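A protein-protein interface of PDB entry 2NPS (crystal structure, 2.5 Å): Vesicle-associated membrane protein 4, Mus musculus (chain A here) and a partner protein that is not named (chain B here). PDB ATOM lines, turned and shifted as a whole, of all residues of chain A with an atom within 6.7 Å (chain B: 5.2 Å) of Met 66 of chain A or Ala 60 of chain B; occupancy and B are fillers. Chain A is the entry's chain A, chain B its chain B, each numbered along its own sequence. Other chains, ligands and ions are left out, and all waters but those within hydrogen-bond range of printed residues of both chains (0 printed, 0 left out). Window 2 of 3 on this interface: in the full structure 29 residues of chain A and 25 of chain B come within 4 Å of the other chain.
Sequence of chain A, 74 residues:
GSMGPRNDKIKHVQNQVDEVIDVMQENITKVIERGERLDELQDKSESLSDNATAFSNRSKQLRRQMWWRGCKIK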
ATOM      1  N   SER A  59     -14.566 -23.555  11.819  1.00  0.00           N
ATOM      2  CA  SER A  59     -13.274 -22.881  11.718  1.00  0.00           C
ATOM      3  C   SER A  59     -13.297 -21.540  12.466  1.00  0.00           C
ATOM      4  O   SER A  59     -12.308 -21.151  13.090  1.00  0.00           O
ATOM      5  CB  SER A  59     -12.910 -22.647  10.263  1.00  0.00           C
ATOM      6  OG  SER A  59     -12.703 -23.885   9.633  1.00  0.00           O
ATOM      7  N   GLN A  61     -15.051 -20.963  15.041  1.00  0.00           N
ATOM      8  CA  GLN A  61     -15.001 -21.350  16.452  1.00  0.00           C
ATOM      9  C   GLN A  61     -13.599 -21.718  16.842  1.00  0.00           C
ATOM     10  O   GLN A  61     -13.145 -21.383  17.928  1.00  0.00           O
ATOM     11  CB  GLN A  61     -15.905 -22.538  16.736  1.00  0.00           C
ATOM     12  CG  GLN A  61     -17.313 -22.358  16.252  1.00  0.00           C
ATOM     13  CD  GLN A  61     -18.193 -23.559  16.566  1.00  0.00           C
ATOM     14  OE1 GLN A  61     -17.695 -24.668  16.788  1.00  0.00           O
ATOM     15  NE2 GLN A  61     -19.507 -23.345  16.572  1.00  0.00           N
ATOM     16  N   LEU A  62     -12.904 -22.408  15.949  1.00  0.00           N
ATOM     17  CA  LEU A  62     -11.536 -22.808  16.231  1.00  0.00           C
ATOM     18  C   LEU A  62     -10.656 -21.577  16.470  1.00  0.00           C
ATOM     19  O   LEU A  62      -9.828 -21.563  17.380  1.00  0.00           O
ATOM     20  CB  LEU A  62     -10.986 -23.643  15.081  1.00  0.00           C
ATOM     21  CG  LEU A  62      -9.599 -24.179  15.380  1.00  0.00           C
ATOM     22  CD1 LEU A  62      -9.658 -24.968  16.665  1.00  0.00           C
ATOM     23  CD2 LEU A  62      -9.118 -25.030  14.247  1.00  0.00           C
ATOM     24  N   ARG A  63     -10.845 -20.553  15.641  1.00  0.00           N
ATOM     25  CA  ARG A  63     -10.128 -19.284  15.763  1.00  0.00           C
ATOM     26  C   ARG A  63     -10.448 -18.611  17.111  1.00  0.00           C
ATOM     27  O   ARG A  63      -9.550 -18.192  17.829  1.00  0.00           O
ATOM     28  CB  ARG A  63     -10.536 -18.344  14.622  1.00  0.00           C
ATOM     29  CG  ARG A  63     -10.092 -16.884  14.764  1.00  0.00           C
ATOM     30  CD  ARG A  63     -11.124 -15.964  14.102  1.00  0.00           C
ATOM     31  NE  ARG A  63     -12.129 -15.511  15.063  1.00  0.00           N
ATOM     32  CZ  ARG A  63     -13.351 -15.067  14.755  1.00  0.00           C
ATOM     33  NH1 ARG A  63     -14.166 -14.677  15.725  1.00  0.00           N
ATOM     34  NH2 ARG A  63     -13.771 -15.021  13.493  1.00  0.00           N
ATOM     35  N   ARG A  64     -11.725 -18.502  17.458  1.00  0.00           N
ATOM     36  CA  ARG A  64     -12.079 -17.885  18.730  1.00  0.00           C
ATOM     37  C   ARG A  64     -11.525 -18.719  19.874  1.00  0.00           C
ATOM     38  O   ARG A  64     -10.996 -18.194  20.840  1.00  0.00           O
ATOM     39  CB  ARG A  64     -13.602 -17.733  18.854  1.00  0.00           C
ATOM     40  CG  ARG A  64     -14.185 -16.756  17.821  1.00  0.00           C
ATOM     41  CD  ARG A  64     -15.637 -16.367  18.077  1.00  0.00           C
ATOM     42  NE  ARG A  64     -16.610 -17.265  17.464  1.00  0.00           N
ATOM     43  CZ  ARG A  64     -17.212 -17.040  16.301  1.00  0.00           C
ATOM     44  NH1 ARG A  64     -18.088 -17.902  15.821  1.00  0.00           N
ATOM     45  NH2 ARG A  64     -16.946 -15.948  15.612  1.00  0.00           N
ATOM     46  N   GLN A  65     -11.613 -20.028  19.741  1.00  0.00           N
ATOM     47  CA  GLN A  65     -11.123 -20.927  20.768  1.00  0.00           C
ATOM     48  C   GLN A  65      -9.603 -20.815  20.918  1.00  0.00           C
ATOM     49  O   GLN A  65      -9.070 -20.889  22.024  1.00  0.00           O
ATOM     50  CB  GLN A  65     -11.538 -22.337  20.392  1.00  0.00           C
ATOM     51  CG  GLN A  65     -11.162 -23.419  21.349  1.00  0.00           C
ATOM     52  CD  GLN A  65     -11.460 -24.773  20.756  1.00  0.00           C
ATOM     53  OE1 GLN A  65     -10.873 -25.770  21.143  1.00  0.00           O
ATOM     54  NE2 GLN A  65     -12.391 -24.812  19.808  1.00  0.00           N
ATOM     55  N   MET A  66      -8.902 -20.634  19.804  1.00  0.00           N
ATOM     56  CA  MET A  66      -7.449 -20.479  19.831  1.00  0.00           C
ATOM     57  C   MET A  66      -7.090 -19.124  20.434  1.00  0.00           C
ATOM     58  O   MET A  66      -5.983 -18.923  20.935  1.00  0.00           O
ATOM     59  CB  MET A  66      -6.852 -20.570  18.418  1.00  0.00           C
ATOM     60  CG  MET A  66      -6.806 -21.970  17.833  1.00  0.00           C
ATOM     61  SD  MET A  66      -6.033 -23.124  18.971  1.00  0.00           S
ATOM     62  CE  MET A  66      -7.470 -23.865  19.708  1.00  0.00           C
ATOM     63  N   TRP A  67      -8.031 -18.187  20.365  1.00  0.00           N
ATOM     64  CA  TRP A  67      -7.824 -16.853  20.920  1.00  0.00           C
ATOM     65  C   TRP A  67      -8.549 -16.814  22.235  1.00  0.00           C
ATOM     66  O   TRP A  67      -9.674 -16.343  22.286  1.00  0.00           O
ATOM     67  CB  TRP A  67      -8.427 -15.769  20.023  1.00  0.00           C
ATOM     68  CG  TRP A  67      -7.870 -14.410  20.326  1.00  0.00           C
ATOM     69  CD1 TRP A  67      -6.906 -13.749  19.614  1.00  0.00           C
ATOM     70  CD2 TRP A  67      -8.146 -13.593  21.477  1.00  0.00           C
ATOM     71  NE1 TRP A  67      -6.547 -12.588  20.257  1.00  0.00           N
ATOM     72  CE2 TRP A  67      -7.281 -12.473  21.422  1.00  0.00           C
ATOM     73  CE3 TRP A  67      -9.007 -13.718  22.590  1.00  0.00           C
ATOM     74  CZ2 TRP A  67      -7.280 -11.460  22.389  1.00  0.00           C
ATOM     75  CZ3 TRP A  67      -9.006 -12.716  23.560  1.00  0.00           C
ATOM     76  CH2 TRP A  67      -8.130 -11.612  23.463  1.00  0.00           C
ATOM     77  N   TRP A  68      -7.914 -17.308  23.293  1.00  0.00           N
ATOM     78  CA  TRP A  68      -8.526 -17.314  24.626  1.00  0.00           C
ATOM     79  C   TRP A  68      -7.749 -18.185  25.597  1.00  0.00           C
ATOM     80  O   TRP A  68      -6.616 -18.596  25.267  1.00  0.00           O
ATOM     81  CB  TRP A  68      -9.981 -17.811  24.580  1.00  0.00           C
ATOM     82  CG  TRP A  68     -11.007 -16.705  24.648  1.00  0.00           C
ATOM     83  CD1 TRP A  68     -11.888 -16.334  23.666  1.00  0.00           C
ATOM     84  CD2 TRP A  68     -11.257 -15.829  25.762  1.00  0.00           C
ATOM     85  NE1 TRP A  68     -12.661 -15.283  24.095  1.00  0.00           N
ATOM     86  CE2 TRP A  68     -12.294 -14.949  25.371  1.00  0.00           C
ATOM     87  CE3 TRP A  68     -10.694 -15.694  27.038  1.00  0.00           C
ATOM     88  CZ2 TRP A  68     -12.795 -13.955  26.230  1.00  0.00           C
ATOM     89  CZ3 TRP A  68     -11.194 -14.701  27.890  1.00  0.00           C
ATOM     90  CH2 TRP A  68     -12.230 -13.842  27.475  1.00  0.00           C
ATOM     91  N   GLN B  56      -9.928 -18.737   8.189  1.00  0.00           N
ATOM     92  CA  GLN B  56     -10.232 -18.729   9.629  1.00  0.00           C
ATOM     93  C   GLN B  56      -9.249 -19.667  10.346  1.00  0.00           C
ATOM     94  O   GLN B  56      -8.931 -19.492  11.521  1.00  0.00           O
ATOM     95  CB  GLN B  56     -11.657 -19.240   9.905  1.00  0.00           C
ATOM     96  CG  GLN B  56     -12.770 -18.303   9.552  1.00  0.00           C
ATOM     97  CD  GLN B  56     -12.525 -16.921  10.103  1.00  0.00           C
ATOM     98  OE1 GLN B  56     -12.404 -16.725  11.321  1.00  0.00           O
ATOM     99  NE2 GLN B  56     -12.429 -15.944   9.207  1.00  0.00           N
ATOM    100  N   LEU B  57      -8.792 -20.681   9.623  1.00  0.00           N
ATOM    101  CA  LEU B  57      -7.861 -21.646  10.172  1.00  0.00           C
ATOM    102  C   LEU B  57      -6.468 -21.061  10.276  1.00  0.00           C
ATOM    103  O   LEU B  57      -5.722 -21.386  11.190  1.00  0.00           O
ATOM    104  CB  LEU B  57      -7.849 -22.900   9.314  1.00  0.00           C
ATOM    105  CG  LEU B  57      -9.064 -23.794   9.515  1.00  0.00           C
ATOM    106  CD1 LEU B  57      -9.038 -24.935   8.544  1.00  0.00           C
ATOM    107  CD2 LEU B  57      -9.075 -24.283  10.921  1.00  0.00           C
ATOM    108  N   GLN B  58      -6.118 -20.192   9.337  1.00  0.00           N
ATOM    109  CA  GLN B  58      -4.811 -19.541   9.373  1.00  0.00           C
ATOM    110  C   GLN B  58      -4.759 -18.602  10.557  1.00  0.00           C
ATOM    111  O   GLN B  58      -3.721 -18.444  11.194  1.00  0.00           O
ATOM    112  CB  GLN B  58      -4.574 -18.734   8.116  1.00  0.00           C
ATOM    113  CG  GLN B  58      -4.404 -19.570   6.887  1.00  0.00           C
ATOM    114  CD  GLN B  58      -3.882 -18.753   5.741  1.00  0.00           C
ATOM    115  OE1 GLN B  58      -4.108 -19.076   4.579  1.00  0.00           O
ATOM    116  NE2 GLN B  58      -3.157 -17.689   6.065  1.00  0.00           N
ATOM    117  N   ARG B  59      -5.888 -17.970  10.836  1.00  0.00           N
ATOM    118  CA  ARG B  59      -5.984 -17.073  11.966  1.00  0.00           C
ATOM    119  C   ARG B  59      -5.931 -17.904  13.250  1.00  0.00           C
ATOM    120  O   ARG B  59      -5.333 -17.499  14.238  1.00  0.00           O
ATOM    121  CB  ARG B  59      -7.294 -16.310  11.922  1.00  0.00           C
ATOM    122  CG  ARG B  59      -7.448 -15.394  10.752  1.00  0.00           C
ATOM    123  CD  ARG B  59      -8.568 -14.425  11.055  1.00  0.00           C
ATOM    124  NE  ARG B  59      -8.503 -13.235  10.225  1.00  0.00           N
ATOM    125  CZ  ARG B  59      -8.800 -13.202   8.930  1.00  0.00           C
ATOM    126  NH1 ARG B  59      -8.706 -12.054   8.261  1.00  0.00           N
ATOM    127  NH2 ARG B  59      -9.200 -14.305   8.302  1.00  0.00           N
ATOM    128  N   ALA B  60      -6.567 -19.072  13.227  1.00  0.00           N
ATOM    129  CA  ALA B  60      -6.563 -19.965  14.386  1.00  0.00           C
ATOM    130  C   ALA B  60      -5.146 -20.409  14.655  1.00  0.00           C
ATOM    131  O   ALA B  60      -4.706 -20.425  15.798  1.00  0.00           O
ATOM    132  CB  ALA B  60      -7.441 -21.181  14.129  1.00  0.00           C
ATOM    133  N   ALA B  61      -4.433 -20.766  13.588  1.00  0.00           N
ATOM    134  CA  ALA B  61      -3.047 -21.214  13.706  1.00  0.00           C
ATOM    135  C   ALA B  61      -2.189 -20.113  14.310  1.00  0.00           C
ATOM    136  O   ALA B  61      -1.452 -20.354  15.254  1.00  0.00           O
ATOM    137  CB  ALA B  61      -2.504 -21.623  12.344  1.00  0.00           C
ATOM    138  N   TYR B  62      -2.296 -18.905  13.764  1.00  0.00           N
ATOM    139  CA  TYR B  62      -1.538 -17.761  14.259  1.00  0.00           C
ATOM    140  C   TYR B  62      -1.736 -17.568  15.751  1.00  0.00           C
ATOM    141  O   TYR B  62      -0.780 -17.379  16.494  1.00  0.00           O
ATOM    142  CB  TYR B  62      -1.981 -16.481  13.558  1.00  0.00           C
ATOM    143  CG  TYR B  62      -1.425 -15.228  14.200  1.00  0.00           C
ATOM    144  CD1 TYR B  62      -0.071 -14.904  14.083  1.00  0.00           C
ATOM    145  CD2 TYR B  62      -2.244 -14.372  14.935  1.00  0.00           C
ATOM    146  CE1 TYR B  62       0.464 -13.757  14.686  1.00  0.00           C
ATOM    147  CE2 TYR B  62      -1.722 -13.215  15.549  1.00  0.00           C
ATOM    148  CZ  TYR B  62      -0.367 -12.917  15.413  1.00  0.00           C
ATOM    149  OH  TYR B  62       0.157 -11.786  15.996  1.00  0.00           O
ATOM    150  N   TYR B  63      -2.995 -17.589  16.171  1.00  0.00           N
ATOM    151  CA  TYR B  63      -3.349 -17.411  17.566  1.00  0.00           C
ATOM    152  C   TYR B  63      -2.797 -18.548  18.404  1.00  0.00           C
ATOM    153  O   TYR B  63      -2.488 -18.370  19.577  1.00  0.00           O
ATOM    154  CB  TYR B  63      -4.866 -17.326  17.706  1.00  0.00           C
ATOM    155  CG  TYR B  63      -5.450 -16.041  17.160  1.00  0.00           C
ATOM    156  CD1 TYR B  63      -6.753 -15.993  16.663  1.00  0.00           C
ATOM    157  CD2 TYR B  63      -4.692 -14.861  17.131  1.00  0.00           C
ATOM    158  CE1 TYR B  63      -7.288 -14.798  16.142  1.00  0.00           C
ATOM    159  CE2 TYR B  63      -5.215 -13.659  16.617  1.00  0.00           C
ATOM    160  CZ  TYR B  63      -6.510 -13.636  16.123  1.00  0.00           C
ATOM    161  OH  TYR B  63      -7.020 -12.458  15.609  1.00  0.00           O
ATOM    162  N   GLN B  64      -2.652 -19.720  17.804  1.00  0.00           N
ATOM    163  CA  GLN B  64      -2.124 -20.839  18.551  1.00  0.00           C
ATOM    164  C   GLN B  64      -0.663 -20.579  18.914  1.00  0.00           C
ATOM    165  O   GLN B  64      -0.237 -20.850  20.034  1.00  0.00           O
ATOM    166  CB  GLN B  64      -2.253 -22.129  17.747  1.00  0.00           C
ATOM    167  CG  GLN B  64      -1.852 -23.361  18.523  1.00  0.00           C
ATOM    168  CD  GLN B  64      -2.053 -24.625  17.733  1.00  0.00           C
ATOM    169  OE1 GLN B  64      -1.595 -24.747  16.597  1.00  0.00           O
ATOM    170  NE2 GLN B  64      -2.740 -25.582  18.330  1.00  0.00           N
ATOM    171  N   SER B  67       0.152 -17.767  21.285  1.00  0.00           N
ATOM    172  CA  SER B  67      -0.182 -18.161  22.647  1.00  0.00           C
ATOM    173  C   SER B  67       1.037 -18.754  23.331  1.00  0.00           C
ATOM    174  O   SER B  67       0.927 -19.767  24.024  1.00  0.00           O
ATOM    175  CB  SER B  67      -1.323 -19.190  22.638  1.00  0.00           C
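Printed residues of chain A that touch a printed residue of chain B: Ser 59, Leu 62, Arg 63, Met 66 and Trp 67.
Of the 10 printed residues of chain B, 4 touch a printed residue of chain A.
Printed residues of chain B that touch a printed residue of chain A: Gln 56, Leu 57, Ala 60 and Tyr 63.
Hydrophobic or aromatic side chains of chain B within 4 Å of the printed part of chain A: Leu 57, Ala 60 and Tyr 63.
Along chain B the printed residues that touch a printed residue of chain A span positions 56 to 63.
Among the printed residues, 10 pairs touch across the chains.
Among the printed residues, no Asp or Glu carboxylate lies within 4 Å of a Lys or Arg side-chain nitrogen of the other chain.
The side-chain amide oxygen (OE1) of Gln 56 of chain B is in hydrogen-bond range of the guanidinium group (NH2) of Arg 63 of chain A, at 3.1 Å.
Among the printed residues, merely in contact across the chains: Met 66 of chain A with Ala 60 of chain B (3.3 Å), Leu 62 of chain A with Leu 57 of chain B (3.4 Å), Trp 67 of chain A with Tyr 63 of chain B (3.4 Å), Ser 59 of chain A with Leu 57 of chain B (3.6 Å), Ser 59 of chain A with Gln 56 of chain B (3.6 Å), Arg 63 of chain A with Ala 60 of chain B (3.7 Å), Arg 63 of chain A with Tyr 63 of chain B (3.7 Å), Met 66 of chain A with Tyr 63 of chain B (3.8 Å) and Leu 62 of chain A with Ala 60 of chain B (3.9 Å).
Of the printed residues of chain B, Ser 59 of chain A touches Gln 56 and Leu 57.
Printed residues of chain B within 4 Å of Leu 62 of chain A: Leu 57 and Ala 60.
Met 66 of chain A touches just these residues of chain B: Ala 60 and Tyr 63.
Printed residues of chain B within 4 Å of Trp 67 of chain A: Tyr 63 (3.4 Å).
Printed residues of chain A within 4 Å of Leu 57 of chain B: Ser 59 (3.6 Å) and Leu 62 (3.4 Å).
Arg 59 of chain B touches none of the printed residues of chain A.
Of the printed residues of chain A, Tyr 63 of chain B touches Arg 63 (3.7 Å), Met 66 (3.8 Å) and Trp 67 (3.4 Å).
The nearest residue of chain A that does not touch Ala 60 of chain B is Ser 59 of chain A (5.0 Å).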
